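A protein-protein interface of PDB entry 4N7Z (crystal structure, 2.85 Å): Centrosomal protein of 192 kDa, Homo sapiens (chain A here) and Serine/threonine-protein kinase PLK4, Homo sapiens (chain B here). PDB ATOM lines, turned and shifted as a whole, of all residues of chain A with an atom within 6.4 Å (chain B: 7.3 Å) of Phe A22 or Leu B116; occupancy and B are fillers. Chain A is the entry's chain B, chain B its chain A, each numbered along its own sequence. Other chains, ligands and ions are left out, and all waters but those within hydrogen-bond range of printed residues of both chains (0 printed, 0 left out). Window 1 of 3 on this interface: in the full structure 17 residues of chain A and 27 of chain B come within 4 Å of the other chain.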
ATOM      1  N   ASP A  19     -15.775 -16.184   4.941  1.00  0.00           N
ATOM      2  CA  ASP A  19     -15.622 -16.742   6.233  1.00  0.00           C
ATOM      3  C   ASP A  19     -14.959 -15.775   7.197  1.00  0.00           C
ATOM      4  O   ASP A  19     -15.408 -15.643   8.315  1.00  0.00           O
ATOM      5  CB  ASP A  19     -14.788 -18.013   6.097  1.00  0.00           C
ATOM      6  CG  ASP A  19     -15.192 -18.843   4.908  1.00  0.00           C
ATOM      7  OD1 ASP A  19     -14.420 -18.957   3.943  1.00  0.00           O
ATOM      8  OD2 ASP A  19     -16.304 -19.364   4.930  1.00  0.00           O
ATOM      9  N   GLU A  20     -13.939 -15.044   6.763  1.00  0.00           N
ATOM     10  CA  GLU A  20     -12.889 -14.593   7.650  1.00  0.00           C
ATOM     11  C   GLU A  20     -13.390 -13.826   8.825  1.00  0.00           C
ATOM     12  O   GLU A  20     -14.277 -13.022   8.718  1.00  0.00           O
ATOM     13  CB  GLU A  20     -11.871 -13.754   6.919  1.00  0.00           C
ATOM     14  CG  GLU A  20     -11.007 -14.530   5.956  1.00  0.00           C
ATOM     15  CD  GLU A  20      -9.942 -15.377   6.607  1.00  0.00           C
ATOM     16  OE1 GLU A  20     -10.266 -16.258   7.402  1.00  0.00           O
ATOM     17  OE2 GLU A  20      -8.765 -15.190   6.301  1.00  0.00           O
ATOM     18  N   MET A  21     -12.807 -14.106   9.970  1.00  0.00           N
ATOM     19  CA  MET A  21     -13.184 -13.474  11.205  1.00  0.00           C
ATOM     20  C   MET A  21     -12.098 -12.484  11.456  1.00  0.00           C
ATOM     21  O   MET A  21     -10.962 -12.859  11.518  1.00  0.00           O
ATOM     22  CB  MET A  21     -13.123 -14.490  12.339  1.00  0.00           C
ATOM     23  CG  MET A  21     -14.172 -15.584  12.344  1.00  0.00           C
ATOM     24  SD  MET A  21     -14.115 -16.576  13.831  1.00  0.00           S
ATOM     25  CE  MET A  21     -12.371 -16.717  14.091  1.00  0.00           C
ATOM     26  N   PHE A  22     -12.425 -11.221  11.609  1.00  0.00           N
ATOM     27  CA  PHE A  22     -11.400 -10.203  11.777  1.00  0.00           C
ATOM     28  C   PHE A  22     -11.286  -9.545  13.127  1.00  0.00           C
ATOM     29  O   PHE A  22     -10.281  -8.985  13.435  1.00  0.00           O
ATOM     30  CB  PHE A  22     -11.473  -9.143  10.672  1.00  0.00           C
ATOM     31  CG  PHE A  22     -12.858  -8.696  10.337  1.00  0.00           C
ATOM     32  CD1 PHE A  22     -13.300  -8.714   9.050  1.00  0.00           C
ATOM     33  CD2 PHE A  22     -13.698  -8.254  11.300  1.00  0.00           C
ATOM     34  CE1 PHE A  22     -14.562  -8.319   8.739  1.00  0.00           C
ATOM     35  CE2 PHE A  22     -14.957  -7.850  10.991  1.00  0.00           C
ATOM     36  CZ  PHE A  22     -15.387  -7.888   9.712  1.00  0.00           C
ATOM     37  N   TYR A  23     -12.306  -9.655  13.949  1.00  0.00           N
ATOM     38  CA  TYR A  23     -12.306  -8.932  15.194  1.00  0.00           C
ATOM     39  C   TYR A  23     -11.564  -9.711  16.222  1.00  0.00           C
ATOM     40  O   TYR A  23     -12.085 -10.578  16.836  1.00  0.00           O
ATOM     41  CB  TYR A  23     -13.721  -8.692  15.651  1.00  0.00           C
ATOM     42  CG  TYR A  23     -13.877  -7.808  16.840  1.00  0.00           C
ATOM     43  CD1 TYR A  23     -15.111  -7.400  17.243  1.00  0.00           C
ATOM     44  CD2 TYR A  23     -12.813  -7.414  17.567  1.00  0.00           C
ATOM     45  CE1 TYR A  23     -15.273  -6.616  18.332  1.00  0.00           C
ATOM     46  CE2 TYR A  23     -12.966  -6.620  18.656  1.00  0.00           C
ATOM     47  CZ  TYR A  23     -14.196  -6.241  19.027  1.00  0.00           C
ATOM     48  OH  TYR A  23     -14.350  -5.455  20.095  1.00  0.00           O
ATOM     49  N   ASP A  24     -10.329  -9.313  16.424  1.00  0.00           N
ATOM     50  CA  ASP A  24      -9.406  -9.981  17.270  1.00  0.00           C
ATOM     51  C   ASP A  24      -8.945  -8.960  18.224  1.00  0.00           C
ATOM     52  O   ASP A  24      -9.374  -7.862  18.155  1.00  0.00           O
ATOM     53  CB  ASP A  24      -8.264 -10.627  16.472  1.00  0.00           C
ATOM     54  CG  ASP A  24      -7.143  -9.711  16.158  1.00  0.00           C
ATOM     55  OD1 ASP A  24      -6.529  -9.126  17.059  1.00  0.00           O
ATOM     56  OD2 ASP A  24      -6.845  -9.608  14.985  1.00  0.00           O
ATOM     57  N   ASP A  25      -8.045  -9.333  19.096  1.00  0.00           N
ATOM     58  CA  ASP A  25      -7.573  -8.417  20.082  1.00  0.00           C
ATOM     59  C   ASP A  25      -6.641  -7.358  19.546  1.00  0.00           C
ATOM     60  O   ASP A  25      -6.346  -6.401  20.226  1.00  0.00           O
ATOM     61  CB  ASP A  25      -7.033  -9.144  21.288  1.00  0.00           C
ATOM     62  CG  ASP A  25      -8.110  -9.883  22.064  1.00  0.00           C
ATOM     63  OD1 ASP A  25      -9.201  -9.326  22.338  1.00  0.00           O
ATOM     64  OD2 ASP A  25      -7.842 -11.039  22.417  1.00  0.00           O
ATOM     65  N   LEU A  27      -7.554  -5.618  17.011  1.00  0.00           N
ATOM     66  CA  LEU A  27      -8.595  -4.678  16.741  1.00  0.00           C
ATOM     67  C   LEU A  27      -9.193  -4.016  17.942  1.00  0.00           C
ATOM     68  O   LEU A  27      -9.535  -2.887  17.909  1.00  0.00           O
ATOM     69  CB  LEU A  27      -9.662  -5.331  15.885  1.00  0.00           C
ATOM     70  CG  LEU A  27     -10.604  -4.431  15.115  1.00  0.00           C
ATOM     71  CD1 LEU A  27      -9.844  -3.705  14.060  1.00  0.00           C
ATOM     72  CD2 LEU A  27     -11.747  -5.193  14.513  1.00  0.00           C
ATOM     73  N   PHE A  31      -9.749  -0.127  18.760  1.00  0.00           N
ATOM     74  CA  PHE A  31     -11.003   0.381  19.176  1.00  0.00           C
ATOM     75  C   PHE A  31     -10.761   1.099  20.465  1.00  0.00           C
ATOM     76  O   PHE A  31     -11.348   2.104  20.726  1.00  0.00           O
ATOM     77  CB  PHE A  31     -12.017  -0.728  19.297  1.00  0.00           C
ATOM     78  CG  PHE A  31     -12.509  -1.229  17.987  1.00  0.00           C
ATOM     79  CD1 PHE A  31     -12.405  -0.475  16.848  1.00  0.00           C
ATOM     80  CD2 PHE A  31     -13.082  -2.456  17.888  1.00  0.00           C
ATOM     81  CE1 PHE A  31     -12.857  -0.941  15.642  1.00  0.00           C
ATOM     82  CE2 PHE A  31     -13.543  -2.917  16.687  1.00  0.00           C
ATOM     83  CZ  PHE A  31     -13.429  -2.160  15.565  1.00  0.00           C
ATOM     84  N   GLN B  25      -5.550  -4.817   9.349  1.00  0.00           N
ATOM     85  CA  GLN B  25      -6.015  -5.968  10.103  1.00  0.00           C
ATOM     86  C   GLN B  25      -5.772  -7.265   9.366  1.00  0.00           C
ATOM     87  O   GLN B  25      -6.362  -7.502   8.314  1.00  0.00           O
ATOM     88  CB  GLN B  25      -7.504  -5.837  10.377  1.00  0.00           C
ATOM     89  CG  GLN B  25      -8.037  -6.959  11.221  1.00  0.00           C
ATOM     90  CD  GLN B  25      -7.391  -6.985  12.585  1.00  0.00           C
ATOM     91  OE1 GLN B  25      -7.235  -5.947  13.233  1.00  0.00           O
ATOM     92  NE2 GLN B  25      -6.999  -8.176  13.027  1.00  0.00           N
ATOM     93  N   LYS B  26      -4.923  -8.114   9.930  1.00  0.00           N
ATOM     94  CA  LYS B  26      -4.614  -9.399   9.320  1.00  0.00           C
ATOM     95  C   LYS B  26      -5.722 -10.397   9.631  1.00  0.00           C
ATOM     96  O   LYS B  26      -6.303 -10.355  10.712  1.00  0.00           O
ATOM     97  CB  LYS B  26      -3.271  -9.906   9.852  1.00  0.00           C
ATOM     98  CG  LYS B  26      -2.845 -11.308   9.390  1.00  0.00           C
ATOM     99  CD  LYS B  26      -2.562 -11.363   7.885  1.00  0.00           C
ATOM    100  CE  LYS B  26      -1.602 -12.503   7.489  1.00  0.00           C
ATOM    101  NZ  LYS B  26      -1.843 -13.847   8.116  1.00  0.00           N
ATOM    102  N   THR B  27      -6.044 -11.258   8.667  1.00  0.00           N
ATOM    103  CA  THR B  27      -6.846 -12.467   8.912  1.00  0.00           C
ATOM    104  C   THR B  27      -6.157 -13.652   8.240  1.00  0.00           C
ATOM    105  O   THR B  27      -5.118 -13.473   7.602  1.00  0.00           O
ATOM    106  CB  THR B  27      -8.303 -12.334   8.436  1.00  0.00           C
ATOM    107  OG1 THR B  27      -8.341 -11.780   7.120  1.00  0.00           O
ATOM    108  CG2 THR B  27      -9.057 -11.412   9.337  1.00  0.00           C
ATOM    109  N   VAL B  32      -7.368  -6.945   5.449  1.00  0.00           N
ATOM    110  CA  VAL B  32      -8.226  -5.823   5.086  1.00  0.00           C
ATOM    111  C   VAL B  32      -7.625  -4.570   5.683  1.00  0.00           C
ATOM    112  O   VAL B  32      -7.175  -4.588   6.829  1.00  0.00           O
ATOM    113  CB  VAL B  32      -9.684  -6.006   5.557  1.00  0.00           C
ATOM    114  CG1 VAL B  32      -9.756  -6.429   7.020  1.00  0.00           C
ATOM    115  CG2 VAL B  32     -10.450  -4.730   5.331  1.00  0.00           C
ATOM    116  N   GLN B 108     -18.084  -6.980  -0.090  1.00  0.00           N
ATOM    117  CA  GLN B 108     -18.872  -7.135   1.117  1.00  0.00           C
ATOM    118  C   GLN B 108     -18.002  -7.441   2.315  1.00  0.00           C
ATOM    119  O   GLN B 108     -18.404  -7.207   3.444  1.00  0.00           O
ATOM    120  CB  GLN B 108     -19.871  -8.270   0.953  1.00  0.00           C
ATOM    121  CG  GLN B 108     -20.899  -8.054  -0.119  1.00  0.00           C
ATOM    122  CD  GLN B 108     -22.199  -8.755   0.208  1.00  0.00           C
ATOM    123  OE1 GLN B 108     -23.030  -8.231   0.964  1.00  0.00           O
ATOM    124  NE2 GLN B 108     -22.383  -9.955  -0.350  1.00  0.00           N
ATOM    125  N   TYR B 109     -16.818  -7.991   2.077  1.00  0.00           N
ATOM    126  CA  TYR B 109     -15.906  -8.229   3.180  1.00  0.00           C
ATOM    127  C   TYR B 109     -15.376  -6.897   3.700  1.00  0.00           C
ATOM    128  O   TYR B 109     -15.459  -6.620   4.898  1.00  0.00           O
ATOM    129  CB  TYR B 109     -14.762  -9.153   2.767  1.00  0.00           C
ATOM    130  CG  TYR B 109     -13.832  -9.485   3.908  1.00  0.00           C
ATOM    131  CD1 TYR B 109     -14.314 -10.087   5.069  1.00  0.00           C
ATOM    132  CD2 TYR B 109     -12.472  -9.203   3.830  1.00  0.00           C
ATOM    133  CE1 TYR B 109     -13.463 -10.391   6.123  1.00  0.00           C
ATOM    134  CE2 TYR B 109     -11.611  -9.511   4.876  1.00  0.00           C
ATOM    135  CZ  TYR B 109     -12.115 -10.101   6.019  1.00  0.00           C
ATOM    136  OH  TYR B 109     -11.266 -10.403   7.059  1.00  0.00           O
ATOM    137  N   ALA B 110     -14.855  -6.075   2.793  1.00  0.00           N
ATOM    138  CA  ALA B 110     -14.399  -4.727   3.137  1.00  0.00           C
ATOM    139  C   ALA B 110     -15.531  -3.851   3.676  1.00  0.00           C
ATOM    140  O   ALA B 110     -15.340  -3.077   4.621  1.00  0.00           O
ATOM    141  CB  ALA B 110     -13.751  -4.070   1.942  1.00  0.00           C
ATOM    142  N   SER B 111     -16.700  -3.985   3.055  1.00  0.00           N
ATOM    143  CA  SER B 111     -17.885  -3.232   3.423  1.00  0.00           C
ATOM    144  C   SER B 111     -18.272  -3.507   4.869  1.00  0.00           C
ATOM    145  O   SER B 111     -18.512  -2.586   5.658  1.00  0.00           O
ATOM    146  CB  SER B 111     -19.031  -3.621   2.492  1.00  0.00           C
ATOM    147  OG  SER B 111     -20.220  -2.931   2.811  1.00  0.00           O
ATOM    148  N   ARG B 112     -18.317  -4.791   5.191  1.00  0.00           N
ATOM    149  CA  ARG B 112     -18.691  -5.304   6.507  1.00  0.00           C
ATOM    150  C   ARG B 112     -17.646  -4.897   7.555  1.00  0.00           C
ATOM    151  O   ARG B 112     -17.970  -4.706   8.721  1.00  0.00           O
ATOM    152  CB  ARG B 112     -18.793  -6.835   6.403  1.00  0.00           C
ATOM    153  CG  ARG B 112     -19.557  -7.582   7.471  1.00  0.00           C
ATOM    154  CD  ARG B 112     -19.948  -8.996   6.983  1.00  0.00           C
ATOM    155  NE  ARG B 112     -18.810  -9.876   6.698  1.00  0.00           N
ATOM    156  CZ  ARG B 112     -18.361 -10.826   7.522  1.00  0.00           C
ATOM    157  NH1 ARG B 112     -18.949 -11.032   8.697  1.00  0.00           N
ATOM    158  NH2 ARG B 112     -17.316 -11.569   7.170  1.00  0.00           N
ATOM    159  N   PHE B 113     -16.390  -4.755   7.137  1.00  0.00           N
ATOM    160  CA  PHE B 113     -15.342  -4.310   8.043  1.00  0.00           C
ATOM    161  C   PHE B 113     -15.549  -2.847   8.425  1.00  0.00           C
ATOM    162  O   PHE B 113     -15.740  -2.518   9.605  1.00  0.00           O
ATOM    163  CB  PHE B 113     -13.978  -4.476   7.388  1.00  0.00           C
ATOM    164  CG  PHE B 113     -12.839  -3.939   8.215  1.00  0.00           C
ATOM    165  CD1 PHE B 113     -12.577  -4.447   9.484  1.00  0.00           C
ATOM    166  CD2 PHE B 113     -12.013  -2.940   7.716  1.00  0.00           C
ATOM    167  CE1 PHE B 113     -11.511  -3.952  10.261  1.00  0.00           C
ATOM    168  CE2 PHE B 113     -10.948  -2.442   8.476  1.00  0.00           C
ATOM    169  CZ  PHE B 113     -10.697  -2.947   9.752  1.00  0.00           C
ATOM    170  N   VAL B 114     -15.504  -1.986   7.409  1.00  0.00           N
ATOM    171  CA  VAL B 114     -15.779  -0.574   7.578  1.00  0.00           C
ATOM    172  C   VAL B 114     -17.013  -0.315   8.445  1.00  0.00           C
ATOM    173  O   VAL B 114     -16.979   0.492   9.380  1.00  0.00           O
ATOM    174  CB  VAL B 114     -15.995   0.082   6.237  1.00  0.00           C
ATOM    175  CG1 VAL B 114     -16.611   1.458   6.421  1.00  0.00           C
ATOM    176  CG2 VAL B 114     -14.683   0.168   5.491  1.00  0.00           C
ATOM    177  N   GLN B 115     -18.093  -1.014   8.136  1.00  0.00           N
ATOM    178  CA  GLN B 115     -19.320  -0.859   8.889  1.00  0.00           C
ATOM    179  C   GLN B 115     -19.074  -1.086  10.368  1.00  0.00           C
ATOM    180  O   GLN B 115     -19.534  -0.305  11.202  1.00  0.00           O
ATOM    181  CB  GLN B 115     -20.384  -1.829   8.377  1.00  0.00           C
ATOM    182  CG  GLN B 115     -21.784  -1.494   8.840  1.00  0.00           C
ATOM    183  CD  GLN B 115     -22.224  -0.093   8.425  1.00  0.00           C
ATOM    184  OE1 GLN B 115     -21.689   0.493   7.475  1.00  0.00           O
ATOM    185  NE2 GLN B 115     -23.206   0.450   9.142  1.00  0.00           N
ATOM    186  N   LEU B 116     -18.328  -2.142  10.690  1.00  0.00           N
ATOM    187  CA  LEU B 116     -18.003  -2.422  12.084  1.00  0.00           C
ATOM    188  C   LEU B 116     -17.068  -1.358  12.669  1.00  0.00           C
ATOM    189  O   LEU B 116     -17.289  -0.889  13.787  1.00  0.00           O
ATOM    190  CB  LEU B 116     -17.407  -3.822  12.242  1.00  0.00           C
ATOM    191  CG  LEU B 116     -16.653  -4.100  13.553  1.00  0.00           C
ATOM    192  CD1 LEU B 116     -17.571  -4.270  14.783  1.00  0.00           C
ATOM    193  CD2 LEU B 116     -15.755  -5.288  13.373  1.00  0.00           C
ATOM    194  N   VAL B 117     -16.037  -0.975  11.920  1.00  0.00           N
ATOM    195  CA  VAL B 117     -15.179   0.106  12.382  1.00  0.00           C
ATOM    196  C   VAL B 117     -16.003   1.367  12.653  1.00  0.00           C
ATOM    197  O   VAL B 117     -15.859   1.985  13.711  1.00  0.00           O
ATOM    198  CB  VAL B 117     -14.021   0.413  11.416  1.00  0.00           C
ATOM    199  CG1 VAL B 117     -13.255   1.639  11.884  1.00  0.00           C
ATOM    200  CG2 VAL B 117     -13.076  -0.778  11.318  1.00  0.00           C
ATOM    201  N   ARG B 118     -16.874   1.723  11.710  1.00  0.00           N
ATOM    202  CA  ARG B 118     -17.732   2.896  11.861  1.00  0.00           C
ATOM    203  C   ARG B 118     -18.532   2.848  13.159  1.00  0.00           C
ATOM    204  O   ARG B 118     -18.733   3.885  13.800  1.00  0.00           O
ATOM    205  CB  ARG B 118     -18.675   3.066  10.655  1.00  0.00           C
ATOM    206  CG  ARG B 118     -18.105   3.906   9.515  1.00  0.00           C
ATOM    207  CD  ARG B 118     -18.783   3.617   8.167  1.00  0.00           C
ATOM    208  NE  ARG B 118     -20.234   3.808   8.190  1.00  0.00           N
ATOM    209  CZ  ARG B 118     -20.861   4.887   7.726  1.00  0.00           C
ATOM    210  NH1 ARG B 118     -20.166   5.881   7.201  1.00  0.00           N
ATOM    211  NH2 ARG B 118     -22.180   4.978   7.788  1.00  0.00           N
ATOM    212  N   SER B 119     -18.964   1.649  13.558  1.00  0.00           N
ATOM    213  CA  SER B 119     -19.830   1.513  14.730  1.00  0.00           C
ATOM    214  C   SER B 119     -19.049   1.635  16.030  1.00  0.00           C
ATOM    215  O   SER B 119     -19.626   1.673  17.110  1.00  0.00           O
ATOM    216  CB  SER B 119     -20.586   0.190  14.702  1.00  0.00           C
ATOM    217  OG  SER B 119     -19.726  -0.885  15.020  1.00  0.00           O
ATOM    218  N   LYS B 120     -17.751   1.753  15.919  1.00  0.00           N
ATOM    219  CA  LYS B 120     -16.928   1.917  17.082  1.00  0.00           C
ATOM    220  C   LYS B 120     -16.099   3.169  17.064  1.00  0.00           C
ATOM    221  O   LYS B 120     -15.419   3.426  17.985  1.00  0.00           O
ATOM    222  CB  LYS B 120     -16.050   0.676  17.304  1.00  0.00           C
ATOM    223  CG  LYS B 120     -16.808  -0.611  17.505  1.00  0.00           C
ATOM    224  CD  LYS B 120     -16.278  -1.433  18.635  1.00  0.00           C
ATOM    225  CE  LYS B 120     -17.341  -1.787  19.623  1.00  0.00           C
ATOM    226  NZ  LYS B 120     -17.054  -3.056  20.293  1.00  0.00           N
ATOM    227  N   SER B 121     -16.193   3.952  16.008  1.00  0.00           N
ATOM    228  CA  SER B 121     -15.476   5.225  15.848  1.00  0.00           C
ATOM    229  C   SER B 121     -16.318   6.403  16.308  1.00  0.00           C
ATOM    230  O   SER B 121     -17.209   6.831  15.577  1.00  0.00           O
ATOM    231  CB  SER B 121     -15.194   5.468  14.371  1.00  0.00           C
ATOM    232  OG  SER B 121     -14.373   4.476  13.808  1.00  0.00           O
ATOM    233  N   ASN B 138     -21.541   5.110  12.441  1.00  0.00           N
ATOM    234  CA  ASN B 138     -22.275   4.164  11.580  1.00  0.00           C
ATOM    235  C   ASN B 138     -23.667   4.642  11.205  1.00  0.00           C
ATOM    236  O   ASN B 138     -24.670   4.027  11.557  1.00  0.00           O
ATOM    237  CB  ASN B 138     -22.316   2.742  12.169  1.00  0.00           C
ATOM    238  CG  ASN B 138     -22.950   2.692  13.545  1.00  0.00           C
ATOM    239  OD1 ASN B 138     -22.926   3.673  14.292  1.00  0.00           O
ATOM    240  ND2 ASN B 138     -23.521   1.539  13.892  1.00  0.00           N
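The backbone carbonyl oxygen (O) of Val B32 is in hydrogen-bond range of the backbone NH (N) of Gln B25, at 3.0 Å.
OG of Ser B119 sits at hydrogen-bond distance from O of Leu B116, at 2.7 Å.
The side-chain hydroxyl (OH) of Tyr B109 is in hydrogen-bond range of the side-chain hydroxyl (OG1) of Thr B27 (3.2 Å).
Of chain B, only Gln B25, Thr B27, Tyr B109, Phe B113 and Leu B116 come within 4 Å of Phe A22.
Of the printed residues of chain B, Phe A31 touches Lys B120 (3.4 Å).
Lys B26 touches none of the printed residues of chain A.
Printed residues of chain A within 4 Å of Tyr B109: Glu A20 and Phe A22.
Of the printed residues of chain A, Phe B113 touches Phe A22 (3.9 Å).
Of the printed residues of chain A, Leu B116 touches Phe A22.
Ser B119 touches none of the printed residues of chain A.
The nearest residue of chain A that does not touch Leu B116 is Leu A27 (4.2 Å).
The nearest printed residue of chain B that does not touch Tyr A23 is Leu B116 (4.5 Å).
O of Phe A22 sits at hydrogen-bond distance from NE2 of Gln B25, 3.4 Å away.
NE2 of Gln B25 lies within hydrogen-bond range of OD2 of Asp A24 (2.4 Å).
OG1 of Thr B27 touches OE2 of Glu A20, at 3.5 Å.
Glu A20 touches Tyr B109.
O of Glu A20 touches NH2 of Arg B112 (3.7 Å).
Thr B27 touches Met A21.
Tyr B109 touches Phe A22.
Phe B113 touches Phe A22 (CA to CZ, 3.9 Å).
Phe A22 touches Leu B116 (CE2 to CD2, 3.6 Å).
Lys B120 touches Tyr A23 (NZ to OH, 3.6 Å).
Gln B25 touches Leu A27 (OE1 to CD1, 3.5 Å).
Phe A31 touches Lys B120.
Of the 9 printed residues of chain A, 7 touch a printed residue of chain B.
Hydrophobic or aromatic side chains of chain A within 4 Å of the printed part of chain B: Phe A22, Tyr A23, Leu A27 and Phe A31.
Hydrophobic or aromatic side chains of chain B within 4 Å of the printed part of chain A: Tyr B109 and Leu B116.
Among the printed residues, no Asp or Glu carboxylate lies within 4 Å of a Lys or Arg side-chain nitrogen of the other chain.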
